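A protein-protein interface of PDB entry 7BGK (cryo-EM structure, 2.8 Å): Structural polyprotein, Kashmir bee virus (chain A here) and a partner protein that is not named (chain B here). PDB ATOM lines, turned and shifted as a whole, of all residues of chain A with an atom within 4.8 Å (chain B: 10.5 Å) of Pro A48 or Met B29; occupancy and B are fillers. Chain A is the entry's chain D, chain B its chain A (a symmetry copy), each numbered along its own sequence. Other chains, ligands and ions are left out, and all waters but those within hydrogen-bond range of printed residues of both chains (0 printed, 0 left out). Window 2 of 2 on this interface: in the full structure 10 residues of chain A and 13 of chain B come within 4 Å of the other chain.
Among the printed residues, merely in contact across the chains: Trp A55 with Met B29, Pro A48 with Met B29, Trp A55 with Gln B35, Val A49 with Asn B25, Val A53 with Met B29 and Trp A55 with Glu B34.
Of chain B, only Met B29 comes within 4 Å of Pro A48. No residue of chain B comes within 4 Å of Ala A46. Of the printed residues of chain B, Val A49 touches Asn B25. No residue of chain B comes within 4 Å of Thr A50. Printed residues of chain A within 4 Å of Asn B25: Val A49 (3.7 Å). Printed residues of chain A within 4 Å of Gln B35: Trp A55 (3.6 Å). Of the printed residues of chain A, Gly B33 touches Trp A55. Printed residues of chain A within 4 Å of Glu B34: Trp A55. Arg B22 touches none of the printed residues of chain A. The nearest residue of chain B that does not touch Pro A48 is Asn B25 (8.2 Å).
O of Glu B21 lies close to ND2 of Asn B25. O of Glu B34 is in hydrogen-bond range of SG of Cys B32. N of Gly B33 lies within hydrogen-bond range of O of Leu B28, at 2.7 Å.
Hydrophobic or aromatic side chains of chain A within 4 Å of the printed part of chain B: Val A49, Val A53 and Trp A55. Hydrophobic or aromatic side chains of chain B that line the printed part of chain A: Met B29.
The indole nitrogen (NE1) of Trp A55 lies within hydrogen-bond range of the backbone carbonyl oxygen (O) of Gly B33 (3.1 Å).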
ATOM      1  N   ALA A  46      -6.654 -14.005   0.286  1.00  0.00           N
ATOM      2  CA  ALA A  46      -7.595 -15.109   0.173  1.00  0.00           C
ATOM      3  C   ALA A  46      -8.984 -14.544   0.430  1.00  0.00           C
ATOM      4  O   ALA A  46      -9.301 -14.133   1.551  1.00  0.00           O
ATOM      5  CB  ALA A  46      -7.262 -16.219   1.164  1.00  0.00           C
ATOM      6  N   LYS A  47      -9.809 -14.539  -0.612  1.00  0.00           N
ATOM      7  CA  LYS A  47     -11.172 -14.014  -0.557  1.00  0.00           C
ATOM      8  C   LYS A  47     -12.044 -14.907  -1.420  1.00  0.00           C
ATOM      9  O   LYS A  47     -12.582 -14.485  -2.451  1.00  0.00           O
ATOM     10  CB  LYS A  47     -11.229 -12.553  -0.997  1.00  0.00           C
ATOM     11  CG  LYS A  47     -10.876 -11.589   0.112  1.00  0.00           C
ATOM     12  CD  LYS A  47     -11.515 -10.236  -0.073  1.00  0.00           C
ATOM     13  CE  LYS A  47     -11.046  -9.568  -1.336  1.00  0.00           C
ATOM     14  NZ  LYS A  47     -11.741  -8.276  -1.556  1.00  0.00           N
ATOM     15  N   PRO A  48     -12.211 -16.147  -1.021  1.00  0.00           N
ATOM     16  CA  PRO A  48     -13.094 -17.056  -1.744  1.00  0.00           C
ATOM     17  C   PRO A  48     -14.549 -16.651  -1.614  1.00  0.00           C
ATOM     18  O   PRO A  48     -14.877 -15.666  -0.945  1.00  0.00           O
ATOM     19  CB  PRO A  48     -12.809 -18.419  -1.092  1.00  0.00           C
ATOM     20  CG  PRO A  48     -12.395 -18.075   0.266  1.00  0.00           C
ATOM     21  CD  PRO A  48     -11.532 -16.855   0.064  1.00  0.00           C
ATOM     22  N   VAL A  49     -15.430 -17.409  -2.255  1.00  0.00           N
ATOM     23  CA  VAL A  49     -16.872 -17.175  -2.135  1.00  0.00           C
ATOM     24  C   VAL A  49     -17.295 -17.924  -0.880  1.00  0.00           C
ATOM     25  O   VAL A  49     -17.779 -19.057  -0.906  1.00  0.00           O
ATOM     26  CB  VAL A  49     -17.640 -17.626  -3.380  1.00  0.00           C
ATOM     27  CG1 VAL A  49     -19.081 -17.195  -3.294  1.00  0.00           C
ATOM     28  CG2 VAL A  49     -16.998 -17.093  -4.642  1.00  0.00           C
ATOM     29  N   THR A  50     -17.114 -17.254   0.254  1.00  0.00           N
ATOM     30  CA  THR A  50     -17.360 -17.818   1.567  1.00  0.00           C
ATOM     31  C   THR A  50     -17.691 -16.664   2.501  1.00  0.00           C
ATOM     32  O   THR A  50     -17.885 -15.527   2.065  1.00  0.00           O
ATOM     33  CB  THR A  50     -16.120 -18.546   2.103  1.00  0.00           C
ATOM     34  OG1 THR A  50     -15.003 -17.656   2.056  1.00  0.00           O
ATOM     35  CG2 THR A  50     -15.778 -19.750   1.269  1.00  0.00           C
ATOM     36  N   ALA A  52     -15.650 -15.218   4.230  1.00  0.00           N
ATOM     37  CA  ALA A  52     -14.484 -14.358   4.375  1.00  0.00           C
ATOM     38  C   ALA A  52     -14.810 -12.911   4.034  1.00  0.00           C
ATOM     39  O   ALA A  52     -14.308 -11.989   4.684  1.00  0.00           O
ATOM     40  CB  ALA A  52     -13.350 -14.868   3.493  1.00  0.00           C
ATOM     41  N   VAL A  53     -15.633 -12.687   3.013  1.00  0.00           N
ATOM     42  CA  VAL A  53     -16.104 -11.341   2.716  1.00  0.00           C
ATOM     43  C   VAL A  53     -17.265 -11.020   3.644  1.00  0.00           C
ATOM     44  O   VAL A  53     -18.045 -11.898   4.026  1.00  0.00           O
ATOM     45  CB  VAL A  53     -16.500 -11.192   1.234  1.00  0.00           C
ATOM     46  CG1 VAL A  53     -15.328 -11.495   0.342  1.00  0.00           C
ATOM     47  CG2 VAL A  53     -17.645 -12.076   0.896  1.00  0.00           C
ATOM     48  N   TRP A  55     -20.120  -9.001   3.391  1.00  0.00           N
ATOM     49  CA  TRP A  55     -21.508  -9.029   2.944  1.00  0.00           C
ATOM     50  C   TRP A  55     -21.994 -10.449   2.669  1.00  0.00           C
ATOM     51  O   TRP A  55     -23.135 -10.801   3.000  1.00  0.00           O
ATOM     52  CB  TRP A  55     -21.674  -8.144   1.711  1.00  0.00           C
ATOM     53  CG  TRP A  55     -20.870  -8.535   0.534  1.00  0.00           C
ATOM     54  CD1 TRP A  55     -19.626  -8.104   0.217  1.00  0.00           C
ATOM     55  CD2 TRP A  55     -21.265  -9.428  -0.505  1.00  0.00           C
ATOM     56  NE1 TRP A  55     -19.212  -8.678  -0.954  1.00  0.00           N
ATOM     57  CE2 TRP A  55     -20.202  -9.500  -1.416  1.00  0.00           C
ATOM     58  CE3 TRP A  55     -22.411 -10.183  -0.750  1.00  0.00           C
ATOM     59  CZ2 TRP A  55     -20.254 -10.286  -2.550  1.00  0.00           C
ATOM     60  CZ3 TRP A  55     -22.456 -10.962  -1.871  1.00  0.00           C
ATOM     61  CH2 TRP A  55     -21.387 -11.011  -2.759  1.00  0.00           C
ATOM     62  N   GLU B  21     -27.385 -20.245  -7.732  1.00  0.00           N
ATOM     63  CA  GLU B  21     -26.885 -19.534  -6.564  1.00  0.00           C
ATOM     64  C   GLU B  21     -25.371 -19.381  -6.621  1.00  0.00           C
ATOM     65  O   GLU B  21     -24.835 -18.285  -6.419  1.00  0.00           O
ATOM     66  CB  GLU B  21     -27.332 -20.279  -5.306  1.00  0.00           C
ATOM     67  CG  GLU B  21     -27.115 -19.563  -3.980  1.00  0.00           C
ATOM     68  CD  GLU B  21     -25.759 -19.849  -3.358  1.00  0.00           C
ATOM     69  OE1 GLU B  21     -25.216 -20.951  -3.578  1.00  0.00           O
ATOM     70  OE2 GLU B  21     -25.240 -18.973  -2.634  1.00  0.00           O
ATOM     71  N   ARG B  22     -24.668 -20.469  -6.932  1.00  0.00           N
ATOM     72  CA  ARG B  22     -23.211 -20.424  -6.982  1.00  0.00           C
ATOM     73  C   ARG B  22     -22.721 -19.505  -8.092  1.00  0.00           C
ATOM     74  O   ARG B  22     -21.783 -18.727  -7.896  1.00  0.00           O
ATOM     75  CB  ARG B  22     -22.662 -21.834  -7.169  1.00  0.00           C
ATOM     76  CG  ARG B  22     -21.155 -21.908  -7.293  1.00  0.00           C
ATOM     77  CD  ARG B  22     -20.687 -23.299  -7.641  1.00  0.00           C
ATOM     78  NE  ARG B  22     -21.255 -23.786  -8.894  1.00  0.00           N
ATOM     79  CZ  ARG B  22     -20.900 -23.350 -10.098  1.00  0.00           C
ATOM     80  NH1 ARG B  22     -19.975 -22.408 -10.221  1.00  0.00           N
ATOM     81  NH2 ARG B  22     -21.474 -23.856 -11.179  1.00  0.00           N
ATOM     82  N   MET B  23     -23.344 -19.585  -9.266  1.00  0.00           N
ATOM     83  CA  MET B  23     -22.916 -18.766 -10.394  1.00  0.00           C
ATOM     84  C   MET B  23     -23.236 -17.299 -10.162  1.00  0.00           C
ATOM     85  O   MET B  23     -22.430 -16.421 -10.491  1.00  0.00           O
ATOM     86  CB  MET B  23     -23.583 -19.271 -11.664  1.00  0.00           C
ATOM     87  CG  MET B  23     -23.337 -20.736 -11.942  1.00  0.00           C
ATOM     88  SD  MET B  23     -24.685 -21.525 -12.817  1.00  0.00           S
ATOM     89  CE  MET B  23     -24.222 -21.111 -14.478  1.00  0.00           C
ATOM     90  N   ASN B  24     -24.407 -17.014  -9.599  1.00  0.00           N
ATOM     91  CA  ASN B  24     -24.753 -15.649  -9.232  1.00  0.00           C
ATOM     92  C   ASN B  24     -23.757 -15.074  -8.240  1.00  0.00           C
ATOM     93  O   ASN B  24     -23.330 -13.922  -8.372  1.00  0.00           O
ATOM     94  CB  ASN B  24     -26.159 -15.619  -8.651  1.00  0.00           C
ATOM     95  CG  ASN B  24     -27.226 -15.709  -9.704  1.00  0.00           C
ATOM     96  OD1 ASN B  24     -26.947 -15.648 -10.898  1.00  0.00           O
ATOM     97  ND2 ASN B  24     -28.461 -15.843  -9.271  1.00  0.00           N
ATOM     98  N   ASN B  25     -23.389 -15.854  -7.225  1.00  0.00           N
ATOM     99  CA  ASN B  25     -22.388 -15.400  -6.271  1.00  0.00           C
ATOM    100  C   ASN B  25     -21.055 -15.138  -6.954  1.00  0.00           C
ATOM    101  O   ASN B  25     -20.452 -14.078  -6.769  1.00  0.00           O
ATOM    102  CB  ASN B  25     -22.233 -16.434  -5.163  1.00  0.00           C
ATOM    103  CG  ASN B  25     -23.474 -16.566  -4.317  1.00  0.00           C
ATOM    104  OD1 ASN B  25     -24.329 -15.685  -4.298  1.00  0.00           O
ATOM    105  ND2 ASN B  25     -23.578 -17.672  -3.605  1.00  0.00           N
ATOM    106  N   GLU B  26     -20.583 -16.089  -7.758  1.00  0.00           N
ATOM    107  CA  GLU B  26     -19.350 -15.879  -8.508  1.00  0.00           C
ATOM    108  C   GLU B  26     -19.403 -14.585  -9.303  1.00  0.00           C
ATOM    109  O   GLU B  26     -18.408 -13.858  -9.390  1.00  0.00           O
ATOM    110  CB  GLU B  26     -19.101 -17.061  -9.439  1.00  0.00           C
ATOM    111  CG  GLU B  26     -18.677 -18.331  -8.743  1.00  0.00           C
ATOM    112  CD  GLU B  26     -18.588 -19.515  -9.682  1.00  0.00           C
ATOM    113  OE1 GLU B  26     -19.257 -19.493 -10.736  1.00  0.00           O
ATOM    114  OE2 GLU B  26     -17.851 -20.471  -9.364  1.00  0.00           O
ATOM    115  N   ALA B  27     -20.556 -14.282  -9.891  1.00  0.00           N
ATOM    116  CA  ALA B  27     -20.687 -13.068 -10.685  1.00  0.00           C
ATOM    117  C   ALA B  27     -20.638 -11.819  -9.819  1.00  0.00           C
ATOM    118  O   ALA B  27     -20.005 -10.825 -10.188  1.00  0.00           O
ATOM    119  CB  ALA B  27     -21.981 -13.118 -11.483  1.00  0.00           C
ATOM    120  N   LEU B  28     -21.304 -11.844  -8.666  1.00  0.00           N
ATOM    121  CA  LEU B  28     -21.322 -10.670  -7.803  1.00  0.00           C
ATOM    122  C   LEU B  28     -19.962 -10.402  -7.182  1.00  0.00           C
ATOM    123  O   LEU B  28     -19.641  -9.252  -6.867  1.00  0.00           O
ATOM    124  CB  LEU B  28     -22.370 -10.841  -6.719  1.00  0.00           C
ATOM    125  CG  LEU B  28     -23.802 -10.950  -7.216  1.00  0.00           C
ATOM    126  CD1 LEU B  28     -24.647 -11.481  -6.126  1.00  0.00           C
ATOM    127  CD2 LEU B  28     -24.324  -9.613  -7.663  1.00  0.00           C
ATOM    128  N   MET B  29     -19.164 -11.440  -6.979  1.00  0.00           N
ATOM    129  CA  MET B  29     -17.808 -11.287  -6.480  1.00  0.00           C
ATOM    130  C   MET B  29     -16.849 -10.777  -7.540  1.00  0.00           C
ATOM    131  O   MET B  29     -15.660 -10.617  -7.252  1.00  0.00           O
ATOM    132  CB  MET B  29     -17.308 -12.621  -5.930  1.00  0.00           C
ATOM    133  CG  MET B  29     -18.236 -13.276  -4.938  1.00  0.00           C
ATOM    134  SD  MET B  29     -18.181 -12.599  -3.283  1.00  0.00           S
ATOM    135  CE  MET B  29     -16.558 -13.117  -2.806  1.00  0.00           C
ATOM    136  N   ARG B  30     -17.337 -10.517  -8.749  1.00  0.00           N
ATOM    137  CA  ARG B  30     -16.517 -10.003  -9.834  1.00  0.00           C
ATOM    138  C   ARG B  30     -17.045  -8.724 -10.449  1.00  0.00           C
ATOM    139  O   ARG B  30     -16.253  -7.984 -11.043  1.00  0.00           O
ATOM    140  CB  ARG B  30     -16.382 -11.047 -10.946  1.00  0.00           C
ATOM    141  CG  ARG B  30     -15.762 -12.341 -10.522  1.00  0.00           C
ATOM    142  CD  ARG B  30     -16.084 -13.427 -11.487  1.00  0.00           C
ATOM    143  NE  ARG B  30     -15.405 -14.668 -11.143  1.00  0.00           N
ATOM    144  CZ  ARG B  30     -15.839 -15.877 -11.476  1.00  0.00           C
ATOM    145  NH1 ARG B  30     -16.958 -16.026 -12.166  1.00  0.00           N
ATOM    146  NH2 ARG B  30     -15.147 -16.943 -11.115  1.00  0.00           N
ATOM    147  N   GLY B  31     -18.339  -8.437 -10.342  1.00  0.00           N
ATOM    148  CA  GLY B  31     -18.909  -7.296 -11.022  1.00  0.00           C
ATOM    149  C   GLY B  31     -19.801  -6.395 -10.197  1.00  0.00           C
ATOM    150  O   GLY B  31     -20.160  -5.313 -10.664  1.00  0.00           O
ATOM    151  N   CYS B  32     -20.201  -6.818  -9.000  1.00  0.00           N
ATOM    152  CA  CYS B  32     -20.997  -5.964  -8.122  1.00  0.00           C
ATOM    153  C   CYS B  32     -20.283  -5.673  -6.809  1.00  0.00           C
ATOM    154  O   CYS B  32     -20.081  -4.501  -6.474  1.00  0.00           O
ATOM    155  CB  CYS B  32     -22.374  -6.582  -7.865  1.00  0.00           C
ATOM    156  SG  CYS B  32     -23.478  -5.498  -6.957  1.00  0.00           S
ATOM    157  N   GLY B  33     -19.879  -6.697  -6.062  1.00  0.00           N
ATOM    158  CA  GLY B  33     -19.390  -6.502  -4.714  1.00  0.00           C
ATOM    159  C   GLY B  33     -20.439  -6.449  -3.630  1.00  0.00           C
ATOM    160  O   GLY B  33     -20.110  -6.101  -2.492  1.00  0.00           O
ATOM    161  N   GLU B  34     -21.685  -6.780  -3.934  1.00  0.00           N
ATOM    162  CA  GLU B  34     -22.755  -6.772  -2.949  1.00  0.00           C
ATOM    163  C   GLU B  34     -23.923  -7.546  -3.536  1.00  0.00           C
ATOM    164  O   GLU B  34     -23.929  -7.884  -4.721  1.00  0.00           O
ATOM    165  CB  GLU B  34     -23.162  -5.350  -2.557  1.00  0.00           C
ATOM    166  CG  GLU B  34     -23.384  -4.396  -3.710  1.00  0.00           C
ATOM    167  CD  GLU B  34     -23.287  -2.950  -3.308  1.00  0.00           C
ATOM    168  OE1 GLU B  34     -22.751  -2.665  -2.222  1.00  0.00           O
ATOM    169  OE2 GLU B  34     -23.750  -2.094  -4.084  1.00  0.00           O
ATOM    170  N   GLN B  35     -24.888  -7.871  -2.683  1.00  0.00           N
ATOM    171  CA  GLN B  35     -26.045  -8.660  -3.095  1.00  0.00           C
ATOM    172  C   GLN B  35     -27.261  -8.091  -2.380  1.00  0.00           C
ATOM    173  O   GLN B  35     -27.410  -8.261  -1.167  1.00  0.00           O
ATOM    174  CB  GLN B  35     -25.853 -10.151  -2.801  1.00  0.00           C
ATOM    175  CG  GLN B  35     -27.115 -10.989  -2.711  1.00  0.00           C
ATOM    176  CD  GLN B  35     -27.579 -11.508  -4.045  1.00  0.00           C
ATOM    177  OE1 GLN B  35     -27.033 -12.476  -4.569  1.00  0.00           O
ATOM    178  NE2 GLN B  35     -28.592 -10.865  -4.612  1.00  0.00           N
